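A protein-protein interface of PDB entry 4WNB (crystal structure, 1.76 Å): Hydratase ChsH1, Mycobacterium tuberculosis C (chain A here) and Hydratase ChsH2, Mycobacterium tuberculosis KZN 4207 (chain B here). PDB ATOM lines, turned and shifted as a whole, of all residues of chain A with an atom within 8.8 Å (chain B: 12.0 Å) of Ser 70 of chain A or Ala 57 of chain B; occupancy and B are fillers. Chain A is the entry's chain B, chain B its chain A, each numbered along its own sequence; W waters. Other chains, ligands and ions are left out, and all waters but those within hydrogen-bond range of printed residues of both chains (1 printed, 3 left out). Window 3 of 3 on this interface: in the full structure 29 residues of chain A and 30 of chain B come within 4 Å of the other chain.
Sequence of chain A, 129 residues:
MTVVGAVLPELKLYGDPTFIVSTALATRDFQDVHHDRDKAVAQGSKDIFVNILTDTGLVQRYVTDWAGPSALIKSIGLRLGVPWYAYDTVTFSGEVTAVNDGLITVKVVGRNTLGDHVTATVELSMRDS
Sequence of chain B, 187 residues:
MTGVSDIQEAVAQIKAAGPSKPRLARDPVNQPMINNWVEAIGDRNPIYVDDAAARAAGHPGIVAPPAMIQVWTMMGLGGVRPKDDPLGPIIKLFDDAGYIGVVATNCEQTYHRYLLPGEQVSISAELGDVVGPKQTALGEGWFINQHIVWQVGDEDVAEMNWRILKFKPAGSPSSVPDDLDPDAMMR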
ATOM      1  N   THR A  64      30.030 -33.328  10.405  1.00  0.00           N
ATOM      2  CA  THR A  64      29.091 -32.240  10.140  1.00  0.00           C
ATOM      3  C   THR A  64      29.437 -31.495   8.848  1.00  0.00           C
ATOM      4  O   THR A  64      28.558 -30.892   8.228  1.00  0.00           O
ATOM      5  CB  THR A  64      29.016 -31.239  11.300  1.00  0.00           C
ATOM      6  OG1 THR A  64      30.295 -30.625  11.491  1.00  0.00           O
ATOM      7  CG2 THR A  64      28.593 -31.942  12.576  1.00  0.00           C
ATOM      8  N   TRP A  66      30.045 -33.003   6.156  1.00  0.00           N
ATOM      9  CA  TRP A  66      29.270 -33.804   5.210  1.00  0.00           C
ATOM     10  C   TRP A  66      27.774 -33.732   5.483  1.00  0.00           C
ATOM     11  O   TRP A  66      26.983 -33.487   4.573  1.00  0.00           O
ATOM     12  CB  TRP A  66      29.741 -35.262   5.254  1.00  0.00           C
ATOM     13  CG  TRP A  66      28.718 -36.260   4.781  1.00  0.00           C
ATOM     14  CD1 TRP A  66      28.443 -36.599   3.491  1.00  0.00           C
ATOM     15  CD2 TRP A  66      27.841 -37.048   5.600  1.00  0.00           C
ATOM     16  NE1 TRP A  66      27.444 -37.547   3.453  1.00  0.00           N
ATOM     17  CE2 TRP A  66      27.061 -37.840   4.735  1.00  0.00           C
ATOM     18  CE3 TRP A  66      27.642 -37.165   6.980  1.00  0.00           C
ATOM     19  CZ2 TRP A  66      26.100 -38.731   5.205  1.00  0.00           C
ATOM     20  CZ3 TRP A  66      26.686 -38.044   7.444  1.00  0.00           C
ATOM     21  CH2 TRP A  66      25.928 -38.818   6.559  1.00  0.00           C
ATOM     22  N   ALA A  67      27.384 -33.954   6.734  1.00  0.00           N
ATOM     23  CA  ALA A  67      25.967 -34.020   7.096  1.00  0.00           C
ATOM     24  C   ALA A  67      25.300 -32.654   7.072  1.00  0.00           C
ATOM     25  O   ALA A  67      24.106 -32.543   6.795  1.00  0.00           O
ATOM     26  CB  ALA A  67      25.795 -34.659   8.473  1.00  0.00           C
ATOM     27  N   GLY A  68      26.064 -31.613   7.377  1.00  0.00           N
ATOM     28  CA  GLY A  68      25.541 -30.259   7.335  1.00  0.00           C
ATOM     29  C   GLY A  68      25.065 -29.757   8.684  1.00  0.00           C
ATOM     30  O   GLY A  68      25.095 -30.497   9.670  1.00  0.00           O
ATOM     31  N   PRO A  69      24.619 -28.494   8.734  1.00  0.00           N
ATOM     32  CA  PRO A  69      24.263 -27.770   9.963  1.00  0.00           C
ATOM     33  C   PRO A  69      23.123 -28.378  10.764  1.00  0.00           C
ATOM     34  O   PRO A  69      23.089 -28.159  11.977  1.00  0.00           O
ATOM     35  CB  PRO A  69      23.842 -26.389   9.455  1.00  0.00           C
ATOM     36  CG  PRO A  69      24.389 -26.289   8.084  1.00  0.00           C
ATOM     37  CD  PRO A  69      24.417 -27.667   7.534  1.00  0.00           C
ATOM     38  N   SER A  70      22.207 -29.096  10.110  1.00  0.00           N
ATOM     39  CA  SER A  70      21.009 -29.602  10.786  1.00  0.00           C
ATOM     40  C   SER A  70      21.263 -30.899  11.547  1.00  0.00           C
ATOM     41  O   SER A  70      20.411 -31.353  12.321  1.00  0.00           O
ATOM     42  CB  SER A  70      19.865 -29.799   9.781  1.00  0.00           C
ATOM     43  OG  SER A  70      20.144 -30.857   8.884  1.00  0.00           O
ATOM     44  N   ALA A  71      22.437 -31.485  11.326  1.00  0.00           N
ATOM     45  CA  ALA A  71      22.815 -32.719  12.004  1.00  0.00           C
ATOM     46  C   ALA A  71      22.938 -32.495  13.506  1.00  0.00           C
ATOM     47  O   ALA A  71      23.450 -31.472  13.951  1.00  0.00           O
ATOM     48  CB  ALA A  71      24.112 -33.254  11.442  1.00  0.00           C
ATOM     49  N   LEU A  72      22.443 -33.450  14.284  1.00  0.00           N
ATOM     50  CA  LEU A  72      22.550 -33.390  15.732  1.00  0.00           C
ATOM     51  C   LEU A  72      23.462 -34.508  16.174  1.00  0.00           C
ATOM     52  O   LEU A  72      23.120 -35.678  16.031  1.00  0.00           O
ATOM     53  CB  LEU A  72      21.182 -33.529  16.397  1.00  0.00           C
ATOM     54  CG  LEU A  72      20.192 -32.393  16.163  1.00  0.00           C
ATOM     55  CD1 LEU A  72      18.795 -32.871  16.478  1.00  0.00           C
ATOM     56  CD2 LEU A  72      20.553 -31.212  17.036  1.00  0.00           C
ATOM     57  N   ILE A  73      24.629 -34.150  16.698  1.00  0.00           N
ATOM     58  CA  ILE A  73      25.608 -35.138  17.104  1.00  0.00           C
ATOM     59  C   ILE A  73      25.202 -35.771  18.430  1.00  0.00           C
ATOM     60  O   ILE A  73      25.068 -35.066  19.434  1.00  0.00           O
ATOM     61  CB  ILE A  73      27.012 -34.507  17.255  1.00  0.00           C
ATOM     62  CG1 ILE A  73      27.470 -33.888  15.928  1.00  0.00           C
ATOM     63  CG2 ILE A  73      28.010 -35.543  17.788  1.00  0.00           C
ATOM     64  CD1 ILE A  73      27.526 -34.867  14.779  1.00  0.00           C
ATOM     65  N   LYS A  74      25.018 -37.092  18.437  1.00  0.00           N
ATOM     66  CA  LYS A  74      24.546 -37.796  19.628  1.00  0.00           C
ATOM     67  C   LYS A  74      25.688 -38.394  20.456  1.00  0.00           C
ATOM     68  O   LYS A  74      25.657 -38.365  21.692  1.00  0.00           O
ATOM     69  CB  LYS A  74      23.563 -38.904  19.236  1.00  0.00           C
ATOM     70  CG  LYS A  74      22.357 -38.411  18.454  1.00  0.00           C
ATOM     71  CD  LYS A  74      21.607 -37.327  19.218  1.00  0.00           C
ATOM     72  CE  LYS A  74      20.262 -37.032  18.560  1.00  0.00           C
ATOM     73  NZ  LYS A  74      19.441 -36.044  19.324  1.00  0.00           N
ATOM     74  N   ILE A 104      21.769 -42.208  12.370  1.00  0.00           N
ATOM     75  CA  ILE A 104      22.850 -42.570  11.451  1.00  0.00           C
ATOM     76  C   ILE A 104      24.142 -42.887  12.199  1.00  0.00           C
ATOM     77  O   ILE A 104      24.501 -42.183  13.139  1.00  0.00           O
ATOM     78  CB  ILE A 104      23.142 -41.430  10.437  1.00  0.00           C
ATOM     79  CG1 ILE A 104      21.844 -40.912   9.808  1.00  0.00           C
ATOM     80  CG2 ILE A 104      24.138 -41.884   9.367  1.00  0.00           C
ATOM     81  CD1 ILE A 104      21.253 -39.697  10.518  1.00  0.00           C
ATOM     82  N   LEU A 124      24.457 -39.702  14.964  1.00  0.00           N
ATOM     83  CA  LEU A 124      23.791 -38.413  14.783  1.00  0.00           C
ATOM     84  C   LEU A 124      22.358 -38.543  14.252  1.00  0.00           C
ATOM     85  O   LEU A 124      21.973 -39.593  13.744  1.00  0.00           O
ATOM     86  CB  LEU A 124      24.599 -37.528  13.826  1.00  0.00           C
ATOM     87  CG  LEU A 124      24.643 -37.974  12.358  1.00  0.00           C
ATOM     88  CD1 LEU A 124      24.809 -36.767  11.442  1.00  0.00           C
ATOM     89  CD2 LEU A 124      25.752 -38.986  12.105  1.00  0.00           C
ATOM     90  N   SER A 125      21.585 -37.465  14.396  1.00  0.00           N
ATOM     91  CA  SER A 125      20.302 -37.288  13.710  1.00  0.00           C
ATOM     92  C   SER A 125      20.499 -36.523  12.404  1.00  0.00           C
ATOM     93  O   SER A 125      21.619 -36.110  12.079  1.00  0.00           O
ATOM     94  CB  SER A 125      19.308 -36.528  14.586  1.00  0.00           C
ATOM     95  OG  SER A 125      18.741 -37.363  15.573  1.00  0.00           O
ATOM     96  N   MET A 126      19.401 -36.304  11.684  1.00  0.00           N
ATOM     97  CA  MET A 126      19.441 -35.660  10.375  1.00  0.00           C
ATOM     98  C   MET A 126      20.040 -34.263  10.451  1.00  0.00           C
ATOM     99  O   MET A 126      20.776 -33.850   9.555  1.00  0.00           O
ATOM    100  CB  MET A 126      18.039 -35.589   9.764  1.00  0.00           C
ATOM    101  CG  MET A 126      18.016 -35.058   8.337  1.00  0.00           C
ATOM    102  SD  MET A 126      16.419 -35.233   7.502  1.00  0.00           S
ATOM    103  CE  MET A 126      16.174 -37.009   7.576  1.00  0.00           C
ATOM    104  N   ASP B  43      36.496 -25.683  12.168  1.00  0.00           N
ATOM    105  CA  ASP B  43      35.070 -26.039  11.955  1.00  0.00           C
ATOM    106  C   ASP B  43      34.205 -24.811  11.675  1.00  0.00           C
ATOM    107  O   ASP B  43      33.952 -24.016  12.574  1.00  0.00           O
ATOM    108  CB  ASP B  43      34.520 -26.770  13.182  1.00  0.00           C
ATOM    109  CG  ASP B  43      33.233 -27.511  12.904  1.00  0.00           C
ATOM    110  OD1 ASP B  43      32.593 -27.237  11.867  1.00  0.00           O
ATOM    111  OD2 ASP B  43      32.850 -28.351  13.753  1.00  0.00           O
ATOM    112  N   ARG B  44      33.729 -24.666  10.438  1.00  0.00           N
ATOM    113  CA  ARG B  44      32.982 -23.476  10.036  1.00  0.00           C
ATOM    114  C   ARG B  44      31.463 -23.602  10.204  1.00  0.00           C
ATOM    115  O   ARG B  44      30.715 -22.747   9.720  1.00  0.00           O
ATOM    116  CB  ARG B  44      33.314 -23.123   8.582  1.00  0.00           C
ATOM    117  CG  ARG B  44      34.824 -23.112   8.310  1.00  0.00           C
ATOM    118  CD  ARG B  44      35.221 -22.294   7.088  1.00  0.00           C
ATOM    119  NE  ARG B  44      34.924 -22.968   5.825  1.00  0.00           N
ATOM    120  CZ  ARG B  44      35.758 -23.791   5.194  1.00  0.00           C
ATOM    121  NH1 ARG B  44      36.953 -24.058   5.705  1.00  0.00           N
ATOM    122  NH2 ARG B  44      35.393 -24.349   4.046  1.00  0.00           N
ATOM    123  N   ASN B  45      31.013 -24.640  10.911  1.00  0.00           N
ATOM    124  CA  ASN B  45      29.585 -24.840  11.186  1.00  0.00           C
ATOM    125  C   ASN B  45      28.927 -23.575  11.727  1.00  0.00           C
ATOM    126  O   ASN B  45      29.263 -23.089  12.808  1.00  0.00           O
ATOM    127  CB  ASN B  45      29.400 -26.007  12.168  1.00  0.00           C
ATOM    128  CG  ASN B  45      27.958 -26.532  12.209  1.00  0.00           C
ATOM    129  OD1 ASN B  45      26.994 -25.777  12.024  1.00  0.00           O
ATOM    130  ND2 ASN B  45      27.809 -27.839  12.476  1.00  0.00           N
ATOM    131  N   PRO B  46      27.983 -23.010  10.949  1.00  0.00           N
ATOM    132  CA  PRO B  46      27.383 -21.717  11.286  1.00  0.00           C
ATOM    133  C   PRO B  46      26.677 -21.665  12.629  1.00  0.00           C
ATOM    134  O   PRO B  46      26.589 -20.591  13.215  1.00  0.00           O
ATOM    135  CB  PRO B  46      26.364 -21.499  10.156  1.00  0.00           C
ATOM    136  CG  PRO B  46      26.855 -22.336   9.036  1.00  0.00           C
ATOM    137  CD  PRO B  46      27.545 -23.514   9.638  1.00  0.00           C
ATOM    138  N   ILE B  47      26.171 -22.797  13.116  1.00  0.00           N
ATOM    139  CA  ILE B  47      25.354 -22.769  14.322  1.00  0.00           C
ATOM    140  C   ILE B  47      26.153 -22.438  15.593  1.00  0.00           C
ATOM    141  O   ILE B  47      25.575 -22.039  16.603  1.00  0.00           O
ATOM    142  CB  ILE B  47      24.593 -24.109  14.499  1.00  0.00           C
ATOM    143  CG1 ILE B  47      25.545 -25.235  14.896  1.00  0.00           C
ATOM    144  CG2 ILE B  47      23.904 -24.467  13.200  1.00  0.00           C
ATOM    145  CD1 ILE B  47      24.872 -26.597  15.073  1.00  0.00           C
ATOM    146  N   TYR B  48      27.481 -22.547  15.524  1.00  0.00           N
ATOM    147  CA  TYR B  48      28.330 -22.204  16.668  1.00  0.00           C
ATOM    148  C   TYR B  48      28.615 -20.701  16.753  1.00  0.00           C
ATOM    149  O   TYR B  48      29.077 -20.211  17.790  1.00  0.00           O
ATOM    150  CB  TYR B  48      29.664 -22.970  16.611  1.00  0.00           C
ATOM    151  CG  TYR B  48      29.520 -24.472  16.436  1.00  0.00           C
ATOM    152  CD1 TYR B  48      28.506 -25.174  17.087  1.00  0.00           C
ATOM    153  CD2 TYR B  48      30.382 -25.183  15.605  1.00  0.00           C
ATOM    154  CE1 TYR B  48      28.368 -26.534  16.920  1.00  0.00           C
ATOM    155  CE2 TYR B  48      30.250 -26.535  15.435  1.00  0.00           C
ATOM    156  CZ  TYR B  48      29.234 -27.203  16.093  1.00  0.00           C
ATOM    157  OH  TYR B  48      29.101 -28.556  15.921  1.00  0.00           O
ATOM    158  N   VAL B  49      28.320 -19.962  15.679  1.00  0.00           N
ATOM    159  CA  VAL B  49      28.740 -18.565  15.611  1.00  0.00           C
ATOM    160  C   VAL B  49      27.681 -17.579  15.103  1.00  0.00           C
ATOM    161  O   VAL B  49      27.936 -16.377  15.083  1.00  0.00           O
ATOM    162  CB  VAL B  49      30.018 -18.419  14.733  1.00  0.00           C
ATOM    163  CG1 VAL B  49      31.200 -19.188  15.369  1.00  0.00           C
ATOM    164  CG2 VAL B  49      29.789 -18.929  13.331  1.00  0.00           C
ATOM    165  N   ASP B  50      26.493 -18.063  14.740  1.00  0.00           N
ATOM    166  CA  ASP B  50      25.483 -17.184  14.141  1.00  0.00           C
ATOM    167  C   ASP B  50      24.070 -17.567  14.603  1.00  0.00           C
ATOM    168  O   ASP B  50      23.557 -18.628  14.241  1.00  0.00           O
ATOM    169  CB  ASP B  50      25.604 -17.233  12.616  1.00  0.00           C
ATOM    170  CG  ASP B  50      24.541 -16.412  11.905  1.00  0.00           C
ATOM    171  OD1 ASP B  50      23.835 -15.603  12.551  1.00  0.00           O
ATOM    172  OD2 ASP B  50      24.422 -16.589  10.675  1.00  0.00           O
ATOM    173  N   ASP B  51      23.480 -16.687  15.417  1.00  0.00           N
ATOM    174  CA  ASP B  51      22.184 -16.930  16.069  1.00  0.00           C
ATOM    175  C   ASP B  51      21.119 -17.320  15.052  1.00  0.00           C
ATOM    176  O   ASP B  51      20.313 -18.225  15.287  1.00  0.00           O
ATOM    177  CB  ASP B  51      21.720 -15.688  16.843  1.00  0.00           C
ATOM    178  CG  ASP B  51      22.357 -15.573  18.218  1.00  0.00           C
ATOM    179  OD1 ASP B  51      22.591 -16.619  18.874  1.00  0.00           O
ATOM    180  OD2 ASP B  51      22.625 -14.426  18.647  1.00  0.00           O
ATOM    181  N   ALA B  52      21.135 -16.635  13.913  1.00  0.00           N
ATOM    182  CA  ALA B  52      20.146 -16.856  12.869  1.00  0.00           C
ATOM    183  C   ALA B  52      20.270 -18.255  12.276  1.00  0.00           C
ATOM    184  O   ALA B  52      19.260 -18.934  12.050  1.00  0.00           O
ATOM    185  CB  ALA B  52      20.280 -15.788  11.769  1.00  0.00           C
ATOM    186  N   ALA B  53      21.510 -18.686  12.065  1.00  0.00           N
ATOM    187  CA  ALA B  53      21.818 -19.972  11.441  1.00  0.00           C
ATOM    188  C   ALA B  53      21.549 -21.131  12.392  1.00  0.00           C
ATOM    189  O   ALA B  53      21.222 -22.252  11.975  1.00  0.00           O
ATOM    190  CB  ALA B  53      23.266 -20.003  10.999  1.00  0.00           C
ATOM    191  N   ALA B  54      21.720 -20.849  13.679  1.00  0.00           N
ATOM    192  CA  ALA B  54      21.428 -21.815  14.727  1.00  0.00           C
ATOM    193  C   ALA B  54      19.921 -21.884  14.951  1.00  0.00           C
ATOM    194  O   ALA B  54      19.460 -22.094  16.067  1.00  0.00           O
ATOM    195  CB  ALA B  54      22.120 -21.448  15.976  1.00  0.00           C
ATOM    196  N   ARG B  55      19.163 -21.736  13.872  1.00  0.00           N
ATOM    197  CA  ARG B  55      17.716 -21.831  13.947  1.00  0.00           C
ATOM    198  C   ARG B  55      17.148 -22.547  12.731  1.00  0.00           C
ATOM    199  O   ARG B  55      16.120 -23.205  12.828  1.00  0.00           O
ATOM    200  CB  ARG B  55      17.104 -20.447  14.107  1.00  0.00           C
ATOM    201  CG  ARG B  55      17.321 -19.901  15.503  1.00  0.00           C
ATOM    202  CD  ARG B  55      16.569 -18.619  15.776  1.00  0.00           C
ATOM    203  NE  ARG B  55      16.965 -18.051  17.064  1.00  0.00           N
ATOM    204  CZ  ARG B  55      17.628 -16.905  17.206  1.00  0.00           C
ATOM    205  NH1 ARG B  55      17.952 -16.188  16.132  1.00  0.00           N
ATOM    206  NH2 ARG B  55      17.947 -16.473  18.425  1.00  0.00           N
ATOM    207  N   ALA B  56      17.824 -22.451  11.594  1.00  0.00           N
ATOM    208  CA  ALA B  56      17.396 -23.197  10.416  1.00  0.00           C
ATOM    209  C   ALA B  56      17.618 -24.689  10.652  1.00  0.00           C
ATOM    210  O   ALA B  56      16.920 -25.539  10.081  1.00  0.00           O
ATOM    211  CB  ALA B  56      18.146 -22.727   9.169  1.00  0.00           C
ATOM    212  N   ALA B  57      18.585 -24.999  11.515  1.00  0.00           N
ATOM    213  CA  ALA B  57      18.869 -26.377  11.876  1.00  0.00           C
ATOM    214  C   ALA B  57      18.075 -26.776  13.123  1.00  0.00           C
ATOM    215  O   ALA B  57      18.169 -27.912  13.588  1.00  0.00           O
ATOM    216  CB  ALA B  57      20.363 -26.561  12.108  1.00  0.00           C
ATOM    217  N   GLY B  58      17.339 -25.824  13.690  1.00  0.00           N
ATOM    218  CA  GLY B  58      16.378 -26.141  14.733  1.00  0.00           C
ATOM    219  C   GLY B  58      16.741 -25.844  16.180  1.00  0.00           C
ATOM    220  O   GLY B  58      16.047 -26.307  17.101  1.00  0.00           O
ATOM    221  N   HIS B  59      17.821 -25.092  16.395  1.00  0.00           N
ATOM    222  CA  HIS B  59      18.257 -24.740  17.754  1.00  0.00           C
ATOM    223  C   HIS B  59      17.651 -23.403  18.170  1.00  0.00           C
ATOM    224  O   HIS B  59      17.112 -22.686  17.328  1.00  0.00           O
ATOM    225  CB  HIS B  59      19.796 -24.694  17.834  1.00  0.00           C
ATOM    226  CG  HIS B  59      20.453 -25.969  17.422  1.00  0.00           C
ATOM    227  ND1 HIS B  59      20.622 -27.027  18.286  1.00  0.00           N
ATOM    228  CD2 HIS B  59      20.941 -26.375  16.226  1.00  0.00           C
ATOM    229  CE1 HIS B  59      21.211 -28.022  17.647  1.00  0.00           C
ATOM    230  NE2 HIS B  59      21.414 -27.653  16.394  1.00  0.00           N
ATOM    231  N   PRO B  60      17.714 -23.060  19.469  1.00  0.00           N
ATOM    232  CA  PRO B  60      17.161 -21.760  19.874  1.00  0.00           C
ATOM    233  C   PRO B  60      17.937 -20.573  19.313  1.00  0.00           C
ATOM    234  O   PRO B  60      17.371 -19.687  18.692  1.00  0.00           O
ATOM    235  CB  PRO B  60      17.271 -21.788  21.399  1.00  0.00           C
ATOM    236  CG  PRO B  60      17.377 -23.226  21.756  1.00  0.00           C
ATOM    237  CD  PRO B  60      18.108 -23.878  20.630  1.00  0.00           C
ATOM    238  N   GLY B  61      19.236 -20.566  19.577  1.00  0.00           N
ATOM    239  CA  GLY B  61      20.174 -19.618  18.999  1.00  0.00           C
ATOM    240  C   GLY B  61      21.497 -20.362  18.954  1.00  0.00           C
ATOM    241  O   GLY B  61      21.489 -21.590  18.955  1.00  0.00           O
ATOM    242  N   ILE B  62      22.619 -19.642  18.895  1.00  0.00           N
ATOM    243  CA  ILE B  62      23.944 -20.274  18.906  1.00  0.00           C
ATOM    244  C   ILE B  62      24.053 -21.376  19.957  1.00  0.00           C
ATOM    245  O   ILE B  62      23.701 -21.167  21.122  1.00  0.00           O
ATOM    246  CB  ILE B  62      25.063 -19.239  19.175  1.00  0.00           C
ATOM    247  CG1 ILE B  62      25.213 -18.301  17.977  1.00  0.00           C
ATOM    248  CG2 ILE B  62      26.401 -19.935  19.523  1.00  0.00           C
ATOM    249  CD1 ILE B  62      26.021 -17.037  18.276  1.00  0.00           C
ATOM    250  N   VAL B  63      24.536 -22.539  19.527  1.00  0.00           N
ATOM    251  CA  VAL B  63      24.827 -23.640  20.432  1.00  0.00           C
ATOM    252  C   VAL B  63      26.350 -23.904  20.449  1.00  0.00           C
ATOM    253  O   VAL B  63      27.050 -23.617  19.469  1.00  0.00           O
ATOM    254  CB  VAL B  63      24.075 -24.926  20.029  1.00  0.00           C
ATOM    255  CG1 VAL B  63      22.588 -24.813  20.342  1.00  0.00           C
ATOM    256  CG2 VAL B  63      24.264 -25.236  18.558  1.00  0.00           C
ATOM    257  N   ALA B  64      26.857 -24.421  21.570  1.00  0.00           N
ATOM    258  CA  ALA B  64      28.274 -24.817  21.654  1.00  0.00           C
ATOM    259  C   ALA B  64      28.482 -26.130  20.930  1.00  0.00           C
ATOM    260  O   ALA B  64      27.579 -26.984  20.935  1.00  0.00           O
ATOM    261  CB  ALA B  64      28.730 -24.942  23.105  1.00  0.00           C
ATOM    262  N   PRO B  66      29.227 -29.767  20.539  1.00  0.00           N
ATOM    263  CA  PRO B  66      29.133 -30.854  21.519  1.00  0.00           C
ATOM    264  C   PRO B  66      30.511 -31.302  22.009  1.00  0.00           C
ATOM    265  O   PRO B  66      30.682 -31.527  23.206  1.00  0.00           O
ATOM    266  CB  PRO B  66      28.436 -31.961  20.738  1.00  0.00           C
ATOM    267  CG  PRO B  66      27.551 -31.211  19.772  1.00  0.00           C
ATOM    268  CD  PRO B  66      28.302 -29.944  19.403  1.00  0.00           C
ATOM    269  N   ARG B 113      22.065 -33.286  24.976  1.00  0.00           N
ATOM    270  CA  ARG B 113      21.569 -32.128  24.232  1.00  0.00           C
ATOM    271  C   ARG B 113      22.699 -31.140  23.981  1.00  0.00           C
ATOM    272  O   ARG B 113      23.766 -31.242  24.596  1.00  0.00           O
ATOM    273  CB  ARG B 113      20.452 -31.417  24.988  1.00  0.00           C
ATOM    274  CG  ARG B 113      20.891 -30.749  26.294  1.00  0.00           C
ATOM    275  CD  ARG B 113      19.823 -29.758  26.765  1.00  0.00           C
ATOM    276  NE  ARG B 113      20.058 -29.185  28.095  1.00  0.00           N
ATOM    277  CZ  ARG B 113      20.642 -28.011  28.310  1.00  0.00           C
ATOM    278  NH1 ARG B 113      21.091 -27.298  27.285  1.00  0.00           N
ATOM    279  NH2 ARG B 113      20.805 -27.560  29.548  1.00  0.00           N
ATOM    280  N   TYR B 114      22.445 -30.173  23.098  1.00  0.00           N
ATOM    281  CA  TYR B 114      23.368 -29.057  22.905  1.00  0.00           C
ATOM    282  C   TYR B 114      23.242 -28.027  24.026  1.00  0.00           C
ATOM    283  O   TYR B 114      22.161 -27.820  24.589  1.00  0.00           O
ATOM    284  CB  TYR B 114      23.123 -28.376  21.556  1.00  0.00           C
ATOM    285  CG  TYR B 114      23.627 -29.148  20.362  1.00  0.00           C
ATOM    286  CD1 TYR B 114      23.184 -30.443  20.110  1.00  0.00           C
ATOM    287  CD2 TYR B 114      24.525 -28.577  19.472  1.00  0.00           C
ATOM    288  CE1 TYR B 114      23.644 -31.154  19.018  1.00  0.00           C
ATOM    289  CE2 TYR B 114      24.978 -29.268  18.372  1.00  0.00           C
ATOM    290  CZ  TYR B 114      24.533 -30.558  18.146  1.00  0.00           C
ATOM    291  OH  TYR B 114      24.984 -31.274  17.062  1.00  0.00           O
ATOM    292  N   LEU B 116      23.933 -23.985  25.576  1.00  0.00           N
ATOM    293  CA  LEU B 116      23.806 -22.611  25.109  1.00  0.00           C
ATOM    294  C   LEU B 116      24.769 -21.726  25.869  1.00  0.00           C
ATOM    295  O   LEU B 116      25.009 -21.952  27.042  1.00  0.00           O
ATOM    296  CB  LEU B 116      22.362 -22.109  25.289  1.00  0.00           C
ATOM    297  CG  LEU B 116      21.244 -22.946  24.669  1.00  0.00           C
ATOM    298  CD1 LEU B 116      19.893 -22.566  25.267  1.00  0.00           C
ATOM    299  CD2 LEU B 116      21.210 -22.780  23.162  1.00  0.00           C
HETATM  300  O   HOH W   1      31.405 -28.892   9.905  1.00  0.00           O
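Printed residues of chain A that touch a printed residue of chain B: Thr 64, Pro 69, Ser 70, Ala 71, Leu 72 and Ile 73.
Hydrophobic or aromatic side chains of chain A that line the printed part of chain B: Leu 72 and Ile 73.
Along chain A the printed residues that touch a printed residue of chain B span positions 64 to 73.
Printed residues of chain B that touch a printed residue of chain A: Asn 45, Ile 47, Ala 57, His 59 and Tyr 114.
Among the printed residues, 9 pairs touch across the chains.
Among the printed residues, no Asp or Glu carboxylate lies within 4 Å of a Lys or Arg side-chain nitrogen of the other chain.
Among the printed residues, merely in contact across the chains: Thr 64 of chain A with Asn 45 of chain B (3.8 Å), Pro 69 of chain A with Asn 45 of chain B (3.96 Å), Pro 69 of chain A with Ile 47 of chain B (3.9 Å), Pro 69 of chain A with Ala 57 of chain B (3.2 Å), Ser 70 of chain A with Ala 57 of chain B (3.4 Å), Leu 72 of chain A with His 59 of chain B (3.3 Å) and Leu 72 of chain A with Tyr 114 of chain B (3.5 Å).
Ala 67 of chain A touches none of the printed residues of chain B.
No residue of chain B comes within 4 Å of Gly 68 of chain A.
Pro 69 of chain A touches three residues of chain B.
Ser 70 of chain A touches one residue of chain B.
Ala 71 of chain A touches one residue of chain B.
Printed residues of chain B within 4 Å of Ile 73 of chain A: Tyr 114.
No residue of chain B comes within 4 Å of Met 126 of chain A.
Of chain A, only Pro 69 and Ser 70 come within 4 Å of Ala 57 of chain B.
No residue of chain A comes within 4 Å of Gly 58 of chain B.
Val 63 of chain B touches none of the printed residues of chain A.
Ala 64 of chain B touches none of the printed residues of chain A.
Of the printed residues of chain A, Tyr 114 of chain B touches Ala 71, Leu 72 and Ile 73.
The nearest residue of chain B that does not touch Ser 70 of chain A is Ala 56 of chain B (5.2 Å).
The nearest residue of chain A that does not touch Ala 57 of chain B is Leu 72 of chain A (5.3 Å).
The nearest printed residue of chain A that does not touch Tyr 114 of chain B is Thr 64 of chain A (5.8 Å).
The side-chain amide oxygen of Asn 45 of chain B sits close to the backbone NH of Ile 47 of chain B.
The backbone NH (N) of Val 63 of chain B sits at hydrogen-bond distance from the backbone carbonyl oxygen (O) of Ile 47 of chain B, at 3.1 Å.
O of Met 126 of chain A lies within hydrogen-bond range of OG of Ser 70 of chain A, at 3.1 Å.
N of Ala 71 of chain A lies close to O of Met 126 of chain A, 3.4 Å away.
The backbone NH (N) of Ser 125 of chain A is in hydrogen-bond range of the backbone carbonyl oxygen (O) of Leu 72 of chain A (2.9 Å).
Water W1 bridges OG1 of Thr 64 of chain A and OD1 of Asp 43 of chain B.
OH of Tyr 114 of chain B is in hydrogen-bond range of O of Ala 71 of chain A, at 3.5 Å.
The backbone NH (N) of Ile 73 of chain A lies within hydrogen-bond range of the side-chain hydroxyl (OH) of Tyr 114 of chain B (2.9 Å).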
